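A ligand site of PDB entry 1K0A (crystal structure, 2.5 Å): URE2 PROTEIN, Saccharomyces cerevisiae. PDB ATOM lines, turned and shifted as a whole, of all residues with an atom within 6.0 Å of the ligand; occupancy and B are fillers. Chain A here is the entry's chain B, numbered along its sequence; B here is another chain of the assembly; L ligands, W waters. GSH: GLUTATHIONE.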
ATOM      1  N   HIS A  25      -0.464  18.673   0.536  1.00  0.00           N
ATOM      2  CA  HIS A  25      -1.380  18.013   1.431  1.00  0.00           C
ATOM      3  C   HIS A  25      -2.029  16.905   0.613  1.00  0.00           C
ATOM      4  O   HIS A  25      -2.456  17.114  -0.516  1.00  0.00           O
ATOM      5  CB  HIS A  25      -2.455  18.979   1.927  1.00  0.00           C
ATOM      6  CG  HIS A  25      -3.498  18.322   2.777  1.00  0.00           C
ATOM      7  ND1 HIS A  25      -4.181  17.205   2.361  1.00  0.00           N
ATOM      8  CD2 HIS A  25      -3.963  18.617   4.016  1.00  0.00           C
ATOM      9  CE1 HIS A  25      -5.028  16.829   3.306  1.00  0.00           C
ATOM     10  NE2 HIS A  25      -4.921  17.679   4.314  1.00  0.00           N
ATOM     11  N   SER A  27      -4.729  15.776   0.093  1.00  0.00           N
ATOM     12  CA  SER A  27      -5.983  16.004  -0.604  1.00  0.00           C
ATOM     13  C   SER A  27      -6.052  17.350  -1.338  1.00  0.00           C
ATOM     14  O   SER A  27      -7.145  17.819  -1.675  1.00  0.00           O
ATOM     15  CB  SER A  27      -7.162  15.905   0.368  1.00  0.00           C
ATOM     16  OG  SER A  27      -7.174  16.994   1.268  1.00  0.00           O
ATOM     17  N   ALA A  28      -4.895  17.953  -1.576  1.00  0.00           N
ATOM     18  CA  ALA A  28      -4.820  19.231  -2.258  1.00  0.00           C
ATOM     19  C   ALA A  28      -4.559  19.016  -3.739  1.00  0.00           C
ATOM     20  O   ALA A  28      -3.465  18.621  -4.131  1.00  0.00           O
ATOM     21  CB  ALA A  28      -3.702  20.075  -1.659  1.00  0.00           C
ATOM     22  N   PRO A  29      -5.574  19.242  -4.588  1.00  0.00           N
ATOM     23  CA  PRO A  29      -5.395  19.054  -6.030  1.00  0.00           C
ATOM     24  C   PRO A  29      -4.344  20.016  -6.590  1.00  0.00           C
ATOM     25  O   PRO A  29      -3.682  19.696  -7.577  1.00  0.00           O
ATOM     26  CB  PRO A  29      -6.788  19.318  -6.592  1.00  0.00           C
ATOM     27  CG  PRO A  29      -7.698  18.939  -5.442  1.00  0.00           C
ATOM     28  CD  PRO A  29      -6.980  19.535  -4.269  1.00  0.00           C
ATOM     29  N   ASN A  30      -4.203  21.179  -5.964  1.00  0.00           N
ATOM     30  CA  ASN A  30      -3.218  22.169  -6.399  1.00  0.00           C
ATOM     31  C   ASN A  30      -1.828  21.616  -6.141  1.00  0.00           C
ATOM     32  O   ASN A  30      -0.885  21.925  -6.864  1.00  0.00           O
ATOM     33  CB  ASN A  30      -3.378  23.486  -5.627  1.00  0.00           C
ATOM     34  CG  ASN A  30      -4.795  23.988  -5.600  1.00  0.00           C
ATOM     35  OD1 ASN A  30      -5.631  23.468  -4.868  1.00  0.00           O
ATOM     36  ND2 ASN A  30      -5.069  25.006  -6.401  1.00  0.00           N
ATOM     37  N   LYS A  33      -0.901  19.184  -8.711  1.00  0.00           N
ATOM     38  CA  LYS A  33      -0.721  19.891  -9.971  1.00  0.00           C
ATOM     39  C   LYS A  33       0.771  20.171 -10.105  1.00  0.00           C
ATOM     40  O   LYS A  33       1.327  20.111 -11.195  1.00  0.00           O
ATOM     41  CB  LYS A  33      -1.510  21.207  -9.977  1.00  0.00           C
ATOM     42  CG  LYS A  33      -1.488  21.903 -11.325  1.00  0.00           C
ATOM     43  CD  LYS A  33      -2.430  23.102 -11.390  1.00  0.00           C
ATOM     44  CE  LYS A  33      -1.999  24.200 -10.448  1.00  0.00           C
ATOM     45  NZ  LYS A  33      -2.913  25.368 -10.552  1.00  0.00           N
ATOM     46  N   PHE A  52      -2.489  19.757   8.570  1.00  0.00           N
ATOM     47  CA  PHE A  52      -3.193  20.996   8.906  1.00  0.00           C
ATOM     48  C   PHE A  52      -3.929  20.960  10.231  1.00  0.00           C
ATOM     49  O   PHE A  52      -4.371  21.999  10.735  1.00  0.00           O
ATOM     50  CB  PHE A  52      -4.142  21.380   7.763  1.00  0.00           C
ATOM     51  CG  PHE A  52      -3.419  21.765   6.508  1.00  0.00           C
ATOM     52  CD1 PHE A  52      -2.714  20.810   5.786  1.00  0.00           C
ATOM     53  CD2 PHE A  52      -3.371  23.080   6.093  1.00  0.00           C
ATOM     54  CE1 PHE A  52      -1.950  21.168   4.673  1.00  0.00           C
ATOM     55  CE2 PHE A  52      -2.616  23.451   4.986  1.00  0.00           C
ATOM     56  CZ  PHE A  52      -1.906  22.495   4.276  1.00  0.00           C
ATOM     57  N   HIS A  57       0.814  24.542   8.589  1.00  0.00           N
ATOM     58  CA  HIS A  57       0.782  25.525   7.514  1.00  0.00           C
ATOM     59  C   HIS A  57       0.849  26.926   8.083  1.00  0.00           C
ATOM     60  O   HIS A  57       1.102  27.896   7.365  1.00  0.00           O
ATOM     61  CB  HIS A  57      -0.489  25.372   6.677  1.00  0.00           C
ATOM     62  CG  HIS A  57      -1.757  25.377   7.477  1.00  0.00           C
ATOM     63  ND1 HIS A  57      -2.071  24.377   8.380  1.00  0.00           N
ATOM     64  CD2 HIS A  57      -2.797  26.234   7.492  1.00  0.00           C
ATOM     65  CE1 HIS A  57      -3.253  24.628   8.914  1.00  0.00           C
ATOM     66  NE2 HIS A  57      -3.715  25.752   8.390  1.00  0.00           N
ATOM     67  N   ASN A  66       5.673  30.333   2.399  1.00  0.00           N
ATOM     68  CA  ASN A  66       4.420  30.795   1.820  1.00  0.00           C
ATOM     69  C   ASN A  66       3.740  31.736   2.802  1.00  0.00           C
ATOM     70  O   ASN A  66       3.150  31.291   3.780  1.00  0.00           O
ATOM     71  CB  ASN A  66       3.484  29.627   1.523  1.00  0.00           C
ATOM     72  CG  ASN A  66       2.261  30.052   0.731  1.00  0.00           C
ATOM     73  OD1 ASN A  66       1.925  31.232   0.681  1.00  0.00           O
ATOM     74  ND2 ASN A  66       1.579  29.095   0.128  1.00  0.00           N
ATOM     75  N   ASN A  68       1.079  33.115   2.624  1.00  0.00           N
ATOM     76  CA  ASN A  68      -0.346  32.803   2.662  1.00  0.00           C
ATOM     77  C   ASN A  68      -0.631  31.620   3.596  1.00  0.00           C
ATOM     78  O   ASN A  68      -1.776  31.358   3.955  1.00  0.00           O
ATOM     79  CB  ASN A  68      -0.864  32.480   1.262  1.00  0.00           C
ATOM     80  CG  ASN A  68      -2.386  32.537   1.170  1.00  0.00           C
ATOM     81  OD1 ASN A  68      -2.991  31.904   0.308  1.00  0.00           O
ATOM     82  ND2 ASN A  68      -2.993  33.320   2.036  1.00  0.00           N
ATOM     83  N   ALA A  69       0.424  30.918   3.978  1.00  0.00           N
ATOM     84  CA  ALA A  69       0.283  29.779   4.872  1.00  0.00           C
ATOM     85  C   ALA A  69      -0.627  28.688   4.310  1.00  0.00           C
ATOM     86  O   ALA A  69      -1.527  28.204   4.998  1.00  0.00           O
ATOM     87  CB  ALA A  69      -0.233  30.252   6.230  1.00  0.00           C
ATOM     88  N   ARG A  70      -0.397  28.303   3.051  1.00  0.00           N
ATOM     89  CA  ARG A  70      -1.182  27.255   2.403  1.00  0.00           C
ATOM     90  C   ARG A  70      -0.292  26.483   1.439  1.00  0.00           C
ATOM     91  O   ARG A  70       0.820  26.889   1.138  1.00  0.00           O
ATOM     92  CB  ARG A  70      -2.355  27.863   1.615  1.00  0.00           C
ATOM     93  CG  ARG A  70      -3.214  28.795   2.433  1.00  0.00           C
ATOM     94  CD  ARG A  70      -4.692  28.489   2.270  1.00  0.00           C
ATOM     95  NE  ARG A  70      -5.510  29.295   3.176  1.00  0.00           N
ATOM     96  CZ  ARG A  70      -5.437  29.262   4.508  1.00  0.00           C
ATOM     97  NH1 ARG A  70      -6.223  30.040   5.233  1.00  0.00           N
ATOM     98  NH2 ARG A  70      -4.567  28.451   5.110  1.00  0.00           N
ATOM     99  N   VAL A  71      -0.805  25.355   0.964  1.00  0.00           N
ATOM    100  CA  VAL A  71      -0.058  24.550   0.018  1.00  0.00           C
ATOM    101  C   VAL A  71      -0.789  24.709  -1.313  1.00  0.00           C
ATOM    102  O   VAL A  71      -1.985  25.005  -1.342  1.00  0.00           O
ATOM    103  CB  VAL A  71      -0.033  23.060   0.440  1.00  0.00           C
ATOM    104  CG1 VAL A  71       0.595  22.948   1.815  1.00  0.00           C
ATOM    105  CG2 VAL A  71      -1.435  22.489   0.439  1.00  0.00           C
ATOM    106  N   PRO A  72      -0.083  24.493  -2.444  1.00  0.00           N
ATOM    107  CA  PRO A  72       1.335  24.120  -2.538  1.00  0.00           C
ATOM    108  C   PRO A  72       2.363  25.236  -2.359  1.00  0.00           C
ATOM    109  O   PRO A  72       2.061  26.417  -2.533  1.00  0.00           O
ATOM    110  CB  PRO A  72       1.429  23.514  -3.925  1.00  0.00           C
ATOM    111  CG  PRO A  72       0.482  24.364  -4.706  1.00  0.00           C
ATOM    112  CD  PRO A  72      -0.711  24.471  -3.776  1.00  0.00           C
ATOM    113  N   TRP A  85       5.487  30.236  -4.105  1.00  0.00           N
ATOM    114  CA  TRP A  85       4.171  29.841  -3.621  1.00  0.00           C
ATOM    115  C   TRP A  85       3.131  30.195  -4.673  1.00  0.00           C
ATOM    116  O   TRP A  85       3.405  31.008  -5.555  1.00  0.00           O
ATOM    117  CB  TRP A  85       3.851  30.496  -2.276  1.00  0.00           C
ATOM    118  CG  TRP A  85       4.095  31.973  -2.225  1.00  0.00           C
ATOM    119  CD1 TRP A  85       5.315  32.602  -2.238  1.00  0.00           C
ATOM    120  CD2 TRP A  85       3.118  33.000  -2.105  1.00  0.00           C
ATOM    121  NE1 TRP A  85       5.143  33.962  -2.124  1.00  0.00           N
ATOM    122  CE2 TRP A  85       3.807  34.235  -2.048  1.00  0.00           C
ATOM    123  CE3 TRP A  85       1.709  33.004  -2.036  1.00  0.00           C
ATOM    124  CZ2 TRP A  85       3.141  35.465  -1.925  1.00  0.00           C
ATOM    125  CZ3 TRP A  85       1.050  34.229  -1.924  1.00  0.00           C
ATOM    126  CH2 TRP A  85       1.765  35.441  -1.859  1.00  0.00           C
ATOM    127  N   GLU A  86       1.960  29.563  -4.597  1.00  0.00           N
ATOM    128  CA  GLU A  86       0.872  29.729  -5.570  1.00  0.00           C
ATOM    129  C   GLU A  86       1.139  28.791  -6.753  1.00  0.00           C
ATOM    130  O   GLU A  86       2.034  29.034  -7.567  1.00  0.00           O
ATOM    131  CB  GLU A  86       0.776  31.187  -6.058  1.00  0.00           C
ATOM    132  CG  GLU A  86       0.104  32.118  -5.058  1.00  0.00           C
ATOM    133  CD  GLU A  86      -1.351  31.755  -4.843  1.00  0.00           C
ATOM    134  OE1 GLU A  86      -1.829  31.934  -3.692  1.00  0.00           O
ATOM    135  OE2 GLU A  86      -2.014  31.301  -5.802  1.00  0.00           O
ATOM    136  N   SER A  87       0.374  27.696  -6.826  1.00  0.00           N
ATOM    137  CA  SER A  87       0.538  26.703  -7.895  1.00  0.00           C
ATOM    138  C   SER A  87       0.727  27.307  -9.291  1.00  0.00           C
ATOM    139  O   SER A  87       1.458  26.760 -10.130  1.00  0.00           O
ATOM    140  CB  SER A  87      -0.648  25.737  -7.876  1.00  0.00           C
ATOM    141  OG  SER A  87      -1.847  26.395  -8.217  1.00  0.00           O
ATOM    142  N   GLY A  88       0.067  28.444  -9.541  1.00  0.00           N
ATOM    143  CA  GLY A  88       0.212  29.093 -10.833  1.00  0.00           C
ATOM    144  C   GLY A  88       1.621  29.653 -11.016  1.00  0.00           C
ATOM    145  O   GLY A  88       2.253  29.470 -12.063  1.00  0.00           O
ATOM    146  N   THR A 126      -6.896  28.536 -12.272  1.00  0.00           N
ATOM    147  CA  THR A 126      -6.570  28.860 -10.889  1.00  0.00           C
ATOM    148  C   THR A 126      -7.496  29.902 -10.244  1.00  0.00           C
ATOM    149  O   THR A 126      -7.613  29.932  -9.023  1.00  0.00           O
ATOM    150  CB  THR A 126      -5.152  29.402 -10.775  1.00  0.00           C
ATOM    151  OG1 THR A 126      -5.043  30.592 -11.562  1.00  0.00           O
ATOM    152  CG2 THR A 126      -4.139  28.380 -11.268  1.00  0.00           C
ATOM    153  N   TRP A 222      -8.292  18.634 -10.531  1.00  0.00           N
ATOM    154  CA  TRP A 222      -9.652  19.034 -10.225  1.00  0.00           C
ATOM    155  C   TRP A 222     -10.679  18.282 -11.060  1.00  0.00           C
ATOM    156  O   TRP A 222     -11.792  18.003 -10.578  1.00  0.00           O
ATOM    157  CB  TRP A 222      -9.800  20.549 -10.426  1.00  0.00           C
ATOM    158  CG  TRP A 222      -8.918  21.322  -9.493  1.00  0.00           C
ATOM    159  CD1 TRP A 222      -7.638  21.750  -9.732  1.00  0.00           C
ATOM    160  CD2 TRP A 222      -9.229  21.705  -8.145  1.00  0.00           C
ATOM    161  NE1 TRP A 222      -7.138  22.366  -8.609  1.00  0.00           N
ATOM    162  CE2 TRP A 222      -8.085  22.352  -7.624  1.00  0.00           C
ATOM    163  CE3 TRP A 222     -10.367  21.547  -7.331  1.00  0.00           C
ATOM    164  CZ2 TRP A 222      -8.048  22.844  -6.318  1.00  0.00           C
ATOM    165  CZ3 TRP A 222     -10.322  22.047  -6.034  1.00  0.00           C
ATOM    166  CH2 TRP A 222      -9.166  22.683  -5.536  1.00  0.00           C
ATOM    167  N   PHE B 123      -0.735  35.838  -8.725  1.00  0.00           N
ATOM    168  CA  PHE B 123      -1.701  34.748  -8.734  1.00  0.00           C
ATOM    169  C   PHE B 123      -2.517  34.785  -7.464  1.00  0.00           C
ATOM    170  O   PHE B 123      -3.714  34.463  -7.456  1.00  0.00           O
ATOM    171  CB  PHE B 123      -1.017  33.383  -8.822  1.00  0.00           C
ATOM    172  CG  PHE B 123      -0.822  32.903 -10.219  1.00  0.00           C
ATOM    173  CD1 PHE B 123       0.406  33.052 -10.872  1.00  0.00           C
ATOM    174  CD2 PHE B 123      -1.904  32.342 -10.918  1.00  0.00           C
ATOM    175  CE1 PHE B 123       0.568  32.655 -12.189  1.00  0.00           C
ATOM    176  CE2 PHE B 123      -1.745  31.938 -12.243  1.00  0.00           C
ATOM    177  CZ  PHE B 123      -0.513  32.093 -12.888  1.00  0.00           C
ATOM    178  N   SER B 127      -6.476  35.085  -7.660  1.00  0.00           N
ATOM    179  CA  SER B 127      -7.188  33.856  -7.316  1.00  0.00           C
ATOM    180  C   SER B 127      -7.531  33.696  -5.845  1.00  0.00           C
ATOM    181  O   SER B 127      -8.214  32.740  -5.467  1.00  0.00           O
ATOM    182  CB  SER B 127      -6.389  32.635  -7.761  1.00  0.00           C
ATOM    183  OG  SER B 127      -5.428  32.301  -6.788  1.00  0.00           O
ATOM    184  N   GLY B 128      -7.063  34.608  -5.008  1.00  0.00           N
ATOM    185  CA  GLY B 128      -7.342  34.510  -3.587  1.00  0.00           C
ATOM    186  C   GLY B 128      -7.953  35.772  -3.008  1.00  0.00           C
ATOM    187  O   GLY B 128      -8.791  35.711  -2.124  1.00  0.00           O
HETATM  188  N1  GSH L   1      -1.358  28.349  -4.207  1.00  0.00           N
HETATM  189  CA1 GSH L   1      -2.671  27.605  -4.443  1.00  0.00           C
HETATM  190  C1  GSH L   1      -3.436  28.360  -5.465  1.00  0.00           C
HETATM  191  O11 GSH L   1      -4.297  29.402  -5.050  1.00  0.00           O
HETATM  192  O12 GSH L   1      -3.264  28.017  -6.654  1.00  0.00           O
HETATM  193  CB1 GSH L   1      -3.481  27.437  -3.073  1.00  0.00           C
HETATM  194  CG1 GSH L   1      -4.303  26.118  -3.114  1.00  0.00           C
HETATM  195  CD1 GSH L   1      -5.061  25.891  -1.853  1.00  0.00           C
HETATM  196  OE1 GSH L   1      -5.761  26.799  -1.326  1.00  0.00           O
HETATM  197  N2  GSH L   1      -4.934  24.606  -1.385  1.00  0.00           N
HETATM  198  CA2 GSH L   1      -5.629  24.141  -0.170  1.00  0.00           C
HETATM  199  C2  GSH L   1      -4.911  24.527   1.191  1.00  0.00           C
HETATM  200  O2  GSH L   1      -3.751  24.888   1.276  1.00  0.00           O
HETATM  201  CB2 GSH L   1      -5.668  22.567  -0.129  1.00  0.00           C
HETATM  202  SG2 GSH L   1      -7.173  21.890  -0.831  1.00  0.00           S
HETATM  203  N3  GSH L   1      -5.723  24.430   2.284  1.00  0.00           N
HETATM  204  CA3 GSH L   1      -5.313  24.725   3.657  1.00  0.00           C
HETATM  205  C3  GSH L   1      -6.408  25.488   4.398  1.00  0.00           C
HETATM  206  O31 GSH L   1      -6.168  25.784   5.580  1.00  0.00           O
HETATM  207  O32 GSH L   1      -7.455  25.764   3.780  1.00  0.00           O
HETATM  208  O   HOH W   1      -7.045  28.698  -0.169  1.00  0.00           O
HETATM  209  O   HOH W   2      -0.112  27.707  -2.088  1.00  0.00           O
HETATM  210  O   HOH W   3      -4.773  31.947  -3.344  1.00  0.00           O
HETATM  211  O   HOH W   4      -2.267  29.859  -8.425  1.00  0.00           O
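The side-chain amino group of Lys 33 is in hydrogen-bond range of the side-chain hydroxyl of Ser 87, at 2.8 Å.
The backbone carbonyl oxygen (O) of Phe 123 of chain B is in hydrogen-bond range of the side-chain hydroxyl (OG) of Ser 127 of chain B.
ND2 of Asn 66 is in hydrogen-bond range of O of Arg 70, 2.5 Å away.
N1 of the ligand sits close to N of Ser 87 (3.2 Å).
The backbone NH of Val 71 is in hydrogen-bond range of an oxygen (O2) of the ligand, 3.0 Å away.
NH2 of Arg 70 lies within salt-bridge range of O31 of the ligand, at 3.1 Å.
An oxygen (O12) of the ligand sits at hydrogen-bond distance from the side-chain hydroxyl (OG) of Ser 87 (2.7 Å).
The backbone carbonyl oxygen of Val 71 is in hydrogen-bond range of a nitrogen (N2) of the ligand (3.0 Å).
The side-chain carboxylate of Glu 86 is in salt-bridge range of a nitrogen (N1) of the ligand (3.4 Å).
Merely in contact with the ligand: Ala 28 (3.5 Å), Asn 30 (3.3 Å), Phe 52 (3.3 Å), His 57 (3.7 Å), Pro 72 (3.8 Å) and Ser 127 of chain B (3.6 Å).
Of the 23 residues printed, 10 come within 4 Å of the ligand.
Water W4 lies within hydrogen-bond range of O12 of the ligand (2.7 Å), N of Gly 88 (2.9 Å), OE2 of Glu 86 (3.0 Å) and OG of Ser 87 (3.5 Å).
Water W3 lies within hydrogen-bond range of OE1 of Glu 86 and O11 of the ligand.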
